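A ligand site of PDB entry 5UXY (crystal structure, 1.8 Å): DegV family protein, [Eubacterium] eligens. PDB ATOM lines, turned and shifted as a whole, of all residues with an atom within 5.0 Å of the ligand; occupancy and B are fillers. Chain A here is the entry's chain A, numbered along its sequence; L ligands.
Leu 27 touches the ligand (CD2 to C2, 3.5 Å). CD1 of Ile 83 touches C7 of the ligand, at 3.5 Å. Met 87 touches the ligand (CE to C6, 3.5 Å). N of Gly 89 touches O2 of the ligand, 3.7 Å away. Lys 116 touches the ligand (O to C16, 3.99 Å). Ser 117 touches the ligand. Thr 118 touches the ligand. CD2 of Leu 155 touches C13 of the ligand, 3.7 Å away. Ala 190 touches the ligand (CB to C16, 3.6 Å). O of Gly 194 touches C16 of the ligand, 3.7 Å away. Thr 195 touches the ligand. Leu 196 touches the ligand. Tyr 265 touches the ligand (CB to C9, 3.5 Å). CD1 of Ile 272 touches C17 of the ligand (3.8 Å). The nearest printed residue that does not touch the ligand is Thr 84 (4.02 Å).
OG1 of Thr 60 sits at hydrogen-bond distance from OH of Tyr 265 (2.7 Å). The side-chain hydroxyl of Thr 90 lies within hydrogen-bond range of the side-chain hydroxyl of Ser 88, 2.8 Å away. NE of Arg 170 sits at hydrogen-bond distance from O of Met 87, at 2.8 Å. OH of Tyr 265 is in hydrogen-bond range of NH2 of Arg 170 (3.0 Å). N of Arg 170 lies within hydrogen-bond range of O of Leu 165, 2.9 Å away. The backbone carbonyl oxygen (O) of Leu 155 sits at hydrogen-bond distance from the side-chain hydroxyl (OG1) of Thr 189 (2.7 Å). O of Ser 117 is in hydrogen-bond range of N of Thr 84 (2.9 Å). SG of Cys 262 lies within hydrogen-bond range of OG1 of Thr 118 (3.7 Å).
An oxygen (O1) of the ligand sits at hydrogen-bond distance from the side-chain hydroxyl of Thr 60, at 2.5 Å. An oxygen (O2) of the ligand sits at hydrogen-bond distance from the side-chain hydroxyl (OG) of Ser 88 (2.6 Å). The backbone NH (N) of Ala 61 is in hydrogen-bond range of an oxygen (O1) of the ligand (3.5 Å). O2 of the ligand lies within salt-bridge range of NH1 of Arg 170 (3.9 Å).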
ATOM      1  N   LEU A  27     -27.914  34.318  28.187  1.00  0.00           N
ATOM      2  CA  LEU A  27     -28.727  33.786  27.093  1.00  0.00           C
ATOM      3  C   LEU A  27     -29.915  33.014  27.658  1.00  0.00           C
ATOM      4  O   LEU A  27     -29.992  32.753  28.851  1.00  0.00           O
ATOM      5  CB  LEU A  27     -27.884  32.876  26.212  1.00  0.00           C
ATOM      6  CG  LEU A  27     -27.070  33.705  25.174  1.00  0.00           C
ATOM      7  CD1 LEU A  27     -25.804  34.104  25.862  1.00  0.00           C
ATOM      8  CD2 LEU A  27     -26.793  32.952  23.867  1.00  0.00           C
ATOM      9  N   THR A  60     -32.351  28.271  21.519  1.00  0.00           N
ATOM     10  CA  THR A  60     -31.666  29.274  22.311  1.00  0.00           C
ATOM     11  C   THR A  60     -31.829  30.659  21.674  1.00  0.00           C
ATOM     12  O   THR A  60     -32.114  30.796  20.488  1.00  0.00           O
ATOM     13  CB  THR A  60     -30.167  28.953  22.492  1.00  0.00           C
ATOM     14  OG1 THR A  60     -29.528  28.881  21.209  1.00  0.00           O
ATOM     15  CG2 THR A  60     -30.016  27.576  23.218  1.00  0.00           C
ATOM     16  N   ALA A  61     -31.582  31.680  22.490  1.00  0.00           N
ATOM     17  CA  ALA A  61     -31.688  33.067  22.038  1.00  0.00           C
ATOM     18  C   ALA A  61     -30.576  33.898  22.632  1.00  0.00           C
ATOM     19  O   ALA A  61     -30.241  33.748  23.802  1.00  0.00           O
ATOM     20  CB  ALA A  61     -33.038  33.675  22.439  1.00  0.00           C
ATOM     21  N   CYS A  62     -30.076  34.868  21.862  1.00  0.00           N
ATOM     22  CA  CYS A  62     -29.040  35.776  22.381  1.00  0.00           C
ATOM     23  C   CYS A  62     -29.680  36.817  23.312  1.00  0.00           C
ATOM     24  O   CYS A  62     -30.925  36.948  23.360  1.00  0.00           O
ATOM     25  CB  CYS A  62     -28.312  36.412  21.201  1.00  0.00           C
ATOM     26  SG  CYS A  62     -29.347  37.551  20.324  1.00  0.00           S
ATOM     27  N   ILE A  83     -19.655  34.897  22.616  1.00  0.00           N
ATOM     28  CA  ILE A  83     -19.514  33.618  21.909  1.00  0.00           C
ATOM     29  C   ILE A  83     -19.356  33.885  20.392  1.00  0.00           C
ATOM     30  O   ILE A  83     -19.729  34.946  19.871  1.00  0.00           O
ATOM     31  CB  ILE A  83     -20.759  32.790  22.277  1.00  0.00           C
ATOM     32  CG1 ILE A  83     -20.772  31.431  21.575  1.00  0.00           C
ATOM     33  CG2 ILE A  83     -21.979  33.524  21.918  1.00  0.00           C
ATOM     34  CD1 ILE A  83     -21.900  30.532  22.133  1.00  0.00           C
ATOM     35  N   THR A  84     -18.753  32.940  19.700  1.00  0.00           N
ATOM     36  CA  THR A  84     -18.415  33.073  18.296  1.00  0.00           C
ATOM     37  C   THR A  84     -19.533  33.659  17.441  1.00  0.00           C
ATOM     38  O   THR A  84     -20.679  33.196  17.454  1.00  0.00           O
ATOM     39  CB  THR A  84     -17.993  31.698  17.721  1.00  0.00           C
ATOM     40  OG1 THR A  84     -17.806  31.860  16.315  1.00  0.00           O
ATOM     41  CG2 THR A  84     -19.073  30.622  18.008  1.00  0.00           C
ATOM     42  N   MET A  87     -21.419  31.171  15.050  1.00  0.00           N
ATOM     43  CA  MET A  87     -22.509  30.252  15.380  1.00  0.00           C
ATOM     44  C   MET A  87     -23.743  30.895  16.011  1.00  0.00           C
ATOM     45  O   MET A  87     -24.731  30.216  16.244  1.00  0.00           O
ATOM     46  CB  MET A  87     -22.000  29.182  16.324  1.00  0.00           C
ATOM     47  CG  MET A  87     -20.791  28.477  15.769  1.00  0.00           C
ATOM     48  SD  MET A  87     -21.262  26.639  15.359  1.00  0.00           S
ATOM     49  CE  MET A  87     -21.399  25.827  17.137  1.00  0.00           C
ATOM     50  N   SER A  88     -23.657  32.191  16.287  1.00  0.00           N
ATOM     51  CA  SER A  88     -24.651  32.852  17.140  1.00  0.00           C
ATOM     52  C   SER A  88     -24.781  34.316  16.759  1.00  0.00           C
ATOM     53  O   SER A  88     -23.798  34.938  16.353  1.00  0.00           O
ATOM     54  CB  SER A  88     -24.227  32.760  18.620  1.00  0.00           C
ATOM     55  OG  SER A  88     -25.044  33.510  19.510  1.00  0.00           O
ATOM     56  N   GLY A  89     -25.994  34.876  16.918  1.00  0.00           N
ATOM     57  CA  GLY A  89     -26.266  36.301  16.825  1.00  0.00           C
ATOM     58  C   GLY A  89     -25.845  37.135  18.033  1.00  0.00           C
ATOM     59  O   GLY A  89     -26.091  38.346  18.078  1.00  0.00           O
ATOM     60  N   THR A  90     -25.181  36.530  19.010  1.00  0.00           N
ATOM     61  CA  THR A  90     -24.772  37.252  20.214  1.00  0.00           C
ATOM     62  C   THR A  90     -23.840  38.412  19.907  1.00  0.00           C
ATOM     63  O   THR A  90     -24.034  39.509  20.435  1.00  0.00           O
ATOM     64  CB  THR A  90     -24.126  36.288  21.213  1.00  0.00           C
ATOM     65  OG1 THR A  90     -25.105  35.315  21.621  1.00  0.00           O
ATOM     66  CG2 THR A  90     -23.671  37.071  22.492  1.00  0.00           C
ATOM     67  N   LYS A 116     -14.539  34.024  18.786  1.00  0.00           N
ATOM     68  CA  LYS A 116     -14.422  32.925  17.829  1.00  0.00           C
ATOM     69  C   LYS A 116     -14.522  31.570  18.525  1.00  0.00           C
ATOM     70  O   LYS A 116     -14.064  30.540  18.000  1.00  0.00           O
ATOM     71  CB  LYS A 116     -13.107  33.038  17.080  1.00  0.00           C
ATOM     72  CG  LYS A 116     -12.922  34.371  16.371  1.00  0.00           C
ATOM     73  CD  LYS A 116     -11.393  34.538  16.093  1.00  0.00           C
ATOM     74  CE  LYS A 116     -11.086  35.431  14.933  1.00  0.00           C
ATOM     75  NZ  LYS A 116      -9.699  35.179  14.423  1.00  0.00           N
ATOM     76  N   SER A 117     -15.141  31.531  19.686  1.00  0.00           N
ATOM     77  CA  SER A 117     -15.186  30.251  20.408  1.00  0.00           C
ATOM     78  C   SER A 117     -16.310  30.298  21.458  1.00  0.00           C
ATOM     79  O   SER A 117     -17.340  30.924  21.223  1.00  0.00           O
ATOM     80  CB  SER A 117     -13.785  30.004  20.993  1.00  0.00           C
ATOM     81  OG  SER A 117     -13.733  28.738  21.643  1.00  0.00           O
ATOM     82  N   THR A 118     -16.099  29.653  22.616  1.00  0.00           N
ATOM     83  CA  THR A 118     -17.147  29.558  23.650  1.00  0.00           C
ATOM     84  C   THR A 118     -16.458  29.148  24.954  1.00  0.00           C
ATOM     85  O   THR A 118     -15.274  28.846  24.978  1.00  0.00           O
ATOM     86  CB  THR A 118     -18.229  28.538  23.275  1.00  0.00           C
ATOM     87  OG1 THR A 118     -19.378  28.766  24.096  1.00  0.00           O
ATOM     88  CG2 THR A 118     -17.725  27.063  23.487  1.00  0.00           C
ATOM     89  N   LEU A 155      -9.259  25.591  21.605  1.00  0.00           N
ATOM     90  CA  LEU A 155     -10.345  24.934  22.332  1.00  0.00           C
ATOM     91  C   LEU A 155     -10.536  23.531  21.774  1.00  0.00           C
ATOM     92  O   LEU A 155     -10.555  23.340  20.554  1.00  0.00           O
ATOM     93  CB  LEU A 155     -11.682  25.722  22.205  1.00  0.00           C
ATOM     94  CG  LEU A 155     -12.879  25.033  22.872  1.00  0.00           C
ATOM     95  CD1 LEU A 155     -13.788  26.129  23.480  1.00  0.00           C
ATOM     96  CD2 LEU A 155     -13.664  24.246  21.815  1.00  0.00           C
ATOM     97  N   CYS A 157     -13.114  19.855  22.521  1.00  0.00           N
ATOM     98  CA  CYS A 157     -14.268  19.429  23.288  1.00  0.00           C
ATOM     99  C   CYS A 157     -14.444  17.939  23.030  1.00  0.00           C
ATOM    100  O   CYS A 157     -13.934  17.394  22.058  1.00  0.00           O
ATOM    101  CB  CYS A 157     -15.543  20.164  22.934  1.00  0.00           C
ATOM    102  SG  CYS A 157     -16.044  20.010  21.222  1.00  0.00           S
ATOM    103  N   LEU A 159     -17.929  15.476  23.194  1.00  0.00           N
ATOM    104  CA  LEU A 159     -19.357  15.507  23.425  1.00  0.00           C
ATOM    105  C   LEU A 159     -19.959  14.125  23.284  1.00  0.00           C
ATOM    106  O   LEU A 159     -19.721  13.456  22.277  1.00  0.00           O
ATOM    107  CB  LEU A 159     -20.065  16.459  22.452  1.00  0.00           C
ATOM    108  CG  LEU A 159     -19.370  17.820  22.379  1.00  0.00           C
ATOM    109  CD1 LEU A 159     -20.190  18.720  21.425  1.00  0.00           C
ATOM    110  CD2 LEU A 159     -19.318  18.411  23.811  1.00  0.00           C
ATOM    111  N   LEU A 165     -27.113  20.656  19.373  1.00  0.00           N
ATOM    112  CA  LEU A 165     -26.412  21.314  18.282  1.00  0.00           C
ATOM    113  C   LEU A 165     -27.050  21.006  16.926  1.00  0.00           C
ATOM    114  O   LEU A 165     -27.263  21.889  16.104  1.00  0.00           O
ATOM    115  CB  LEU A 165     -24.919  20.892  18.249  1.00  0.00           C
ATOM    116  CG  LEU A 165     -24.036  21.461  19.360  1.00  0.00           C
ATOM    117  CD1 LEU A 165     -22.796  20.551  19.526  1.00  0.00           C
ATOM    118  CD2 LEU A 165     -23.609  22.921  19.005  1.00  0.00           C
ATOM    119  N   ARG A 170     -26.344  23.655  14.051  1.00  0.00           N
ATOM    120  CA  ARG A 170     -25.012  24.139  14.375  1.00  0.00           C
ATOM    121  C   ARG A 170     -23.939  23.076  14.183  1.00  0.00           C
ATOM    122  O   ARG A 170     -22.748  23.377  14.350  1.00  0.00           O
ATOM    123  CB  ARG A 170     -25.042  24.688  15.820  1.00  0.00           C
ATOM    124  CG  ARG A 170     -25.633  26.100  15.749  1.00  0.00           C
ATOM    125  CD  ARG A 170     -26.185  26.600  17.008  1.00  0.00           C
ATOM    126  NE  ARG A 170     -26.432  28.022  16.786  1.00  0.00           N
ATOM    127  CZ  ARG A 170     -27.603  28.630  16.981  1.00  0.00           C
ATOM    128  NH1 ARG A 170     -27.707  29.913  16.708  1.00  0.00           N
ATOM    129  NH2 ARG A 170     -28.649  27.964  17.440  1.00  0.00           N
ATOM    130  N   THR A 189     -12.915  20.819  17.740  1.00  0.00           N
ATOM    131  CA  THR A 189     -12.129  22.005  18.083  1.00  0.00           C
ATOM    132  C   THR A 189     -12.856  23.221  17.515  1.00  0.00           C
ATOM    133  O   THR A 189     -13.697  23.109  16.628  1.00  0.00           O
ATOM    134  CB  THR A 189     -10.679  21.914  17.522  1.00  0.00           C
ATOM    135  OG1 THR A 189      -9.821  22.958  18.018  1.00  0.00           O
ATOM    136  CG2 THR A 189     -10.718  21.883  15.982  1.00  0.00           C
ATOM    137  N   ALA A 190     -12.540  24.383  18.058  1.00  0.00           N
ATOM    138  CA  ALA A 190     -13.073  25.607  17.437  1.00  0.00           C
ATOM    139  C   ALA A 190     -12.240  25.896  16.189  1.00  0.00           C
ATOM    140  O   ALA A 190     -10.998  25.916  16.254  1.00  0.00           O
ATOM    141  CB  ALA A 190     -13.023  26.769  18.419  1.00  0.00           C
ATOM    142  N   GLY A 194     -14.487  30.078  13.688  1.00  0.00           N
ATOM    143  CA  GLY A 194     -15.360  30.147  14.840  1.00  0.00           C
ATOM    144  C   GLY A 194     -16.522  29.195  14.701  1.00  0.00           C
ATOM    145  O   GLY A 194     -17.633  29.488  15.195  1.00  0.00           O
ATOM    146  N   THR A 195     -16.302  28.022  14.092  1.00  0.00           N
ATOM    147  CA  THR A 195     -17.317  26.966  14.064  1.00  0.00           C
ATOM    148  C   THR A 195     -16.767  25.695  14.696  1.00  0.00           C
ATOM    149  O   THR A 195     -15.556  25.554  14.926  1.00  0.00           O
ATOM    150  CB  THR A 195     -17.773  26.651  12.633  1.00  0.00           C
ATOM    151  OG1 THR A 195     -16.591  26.286  11.893  1.00  0.00           O
ATOM    152  CG2 THR A 195     -18.433  27.881  11.971  1.00  0.00           C
ATOM    153  N   LEU A 196     -17.673  24.768  14.931  1.00  0.00           N
ATOM    154  CA  LEU A 196     -17.294  23.497  15.548  1.00  0.00           C
ATOM    155  C   LEU A 196     -16.761  22.585  14.440  1.00  0.00           C
ATOM    156  O   LEU A 196     -17.472  22.254  13.499  1.00  0.00           O
ATOM    157  CB  LEU A 196     -18.497  22.848  16.236  1.00  0.00           C
ATOM    158  CG  LEU A 196     -18.243  21.477  16.871  1.00  0.00           C
ATOM    159  CD1 LEU A 196     -17.104  21.510  17.881  1.00  0.00           C
ATOM    160  CD2 LEU A 196     -19.546  21.036  17.564  1.00  0.00           C
ATOM    161  N   LEU A 261     -26.021  27.699  29.031  1.00  0.00           N
ATOM    162  CA  LEU A 261     -25.938  27.639  27.571  1.00  0.00           C
ATOM    163  C   LEU A 261     -24.999  26.503  27.165  1.00  0.00           C
ATOM    164  O   LEU A 261     -25.291  25.710  26.250  1.00  0.00           O
ATOM    165  CB  LEU A 261     -25.424  28.992  27.051  1.00  0.00           C
ATOM    166  CG  LEU A 261     -25.440  29.290  25.550  1.00  0.00           C
ATOM    167  CD1 LEU A 261     -24.272  28.643  24.843  1.00  0.00           C
ATOM    168  CD2 LEU A 261     -26.825  28.870  24.962  1.00  0.00           C
ATOM    169  N   CYS A 262     -23.820  26.472  27.756  1.00  0.00           N
ATOM    170  CA  CYS A 262     -22.887  25.398  27.391  1.00  0.00           C
ATOM    171  C   CYS A 262     -23.447  24.027  27.786  1.00  0.00           C
ATOM    172  O   CYS A 262     -23.257  23.044  27.069  1.00  0.00           O
ATOM    173  CB  CYS A 262     -21.535  25.636  28.042  1.00  0.00           C
ATOM    174  SG  CYS A 262     -20.577  27.012  27.149  1.00  0.00           S
ATOM    175  N   TYR A 265     -25.822  22.899  24.900  1.00  0.00           N
ATOM    176  CA  TYR A 265     -25.194  22.513  23.630  1.00  0.00           C
ATOM    177  C   TYR A 265     -24.122  21.422  23.799  1.00  0.00           C
ATOM    178  O   TYR A 265     -23.967  20.584  22.881  1.00  0.00           O
ATOM    179  CB  TYR A 265     -24.575  23.743  22.946  1.00  0.00           C
ATOM    180  CG  TYR A 265     -25.628  24.525  22.211  1.00  0.00           C
ATOM    181  CD1 TYR A 265     -26.363  23.917  21.162  1.00  0.00           C
ATOM    182  CD2 TYR A 265     -25.916  25.853  22.576  1.00  0.00           C
ATOM    183  CE1 TYR A 265     -27.360  24.624  20.470  1.00  0.00           C
ATOM    184  CE2 TYR A 265     -26.928  26.575  21.873  1.00  0.00           C
ATOM    185  CZ  TYR A 265     -27.619  25.962  20.838  1.00  0.00           C
ATOM    186  OH  TYR A 265     -28.633  26.599  20.153  1.00  0.00           O
ATOM    187  N   ALA A 266     -23.404  21.405  24.913  1.00  0.00           N
ATOM    188  CA  ALA A 266     -22.439  20.307  25.112  1.00  0.00           C
ATOM    189  C   ALA A 266     -23.103  19.015  25.601  1.00  0.00           C
ATOM    190  O   ALA A 266     -22.576  17.907  25.351  1.00  0.00           O
ATOM    191  CB  ALA A 266     -21.331  20.745  26.069  1.00  0.00           C
ATOM    192  N   ILE A 272     -15.440  20.607  27.771  1.00  0.00           N
ATOM    193  CA  ILE A 272     -14.807  21.594  26.881  1.00  0.00           C
ATOM    194  C   ILE A 272     -13.536  22.101  27.542  1.00  0.00           C
ATOM    195  O   ILE A 272     -13.542  22.389  28.742  1.00  0.00           O
ATOM    196  CB  ILE A 272     -15.742  22.778  26.596  1.00  0.00           C
ATOM    197  CG1 ILE A 272     -17.116  22.300  26.229  1.00  0.00           C
ATOM    198  CG2 ILE A 272     -15.134  23.615  25.541  1.00  0.00           C
ATOM    199  CD1 ILE A 272     -18.083  23.527  26.113  1.00  0.00           C
HETATM  200  O1  LIG L   1     -28.880  31.146  20.399  1.00  0.00           O
HETATM  201  C1  LIG L   1     -27.698  31.600  20.268  1.00  0.00           C
HETATM  202  O2  LIG L   1     -27.497  32.597  19.483  1.00  0.00           O
HETATM  203  C2  LIG L   1     -26.561  30.872  21.032  1.00  0.00           C
HETATM  204  C3  LIG L   1     -26.073  29.720  20.105  1.00  0.00           C
HETATM  205  C4  LIG L   1     -24.771  29.094  20.654  1.00  0.00           C
HETATM  206  C5  LIG L   1     -24.271  28.053  19.610  1.00  0.00           C
HETATM  207  C6  LIG L   1     -22.899  27.418  19.884  1.00  0.00           C
HETATM  208  C7  LIG L   1     -22.687  27.172  21.382  1.00  0.00           C
HETATM  209  C8  LIG L   1     -21.491  26.214  21.634  1.00  0.00           C
HETATM  210  C9  LIG L   1     -21.582  25.597  23.039  1.00  0.00           C
HETATM  211  C10 LIG L   1     -20.371  23.193  22.428  1.00  0.00           C
HETATM  212  C11 LIG L   1     -18.840  23.060  22.073  1.00  0.00           C
HETATM  213  C12 LIG L   1     -18.577  23.850  20.767  1.00  0.00           C
HETATM  214  C13 LIG L   1     -17.166  24.433  20.648  1.00  0.00           C
HETATM  215  C14 LIG L   1     -16.887  25.111  19.281  1.00  0.00           C
HETATM  216  C15 LIG L   1     -16.805  26.640  19.461  1.00  0.00           C
HETATM  217  C16 LIG L   1     -16.598  27.462  18.171  1.00  0.00           C
HETATM  218  C17 LIG L   1     -20.593  24.434  23.349  1.00  0.00           C
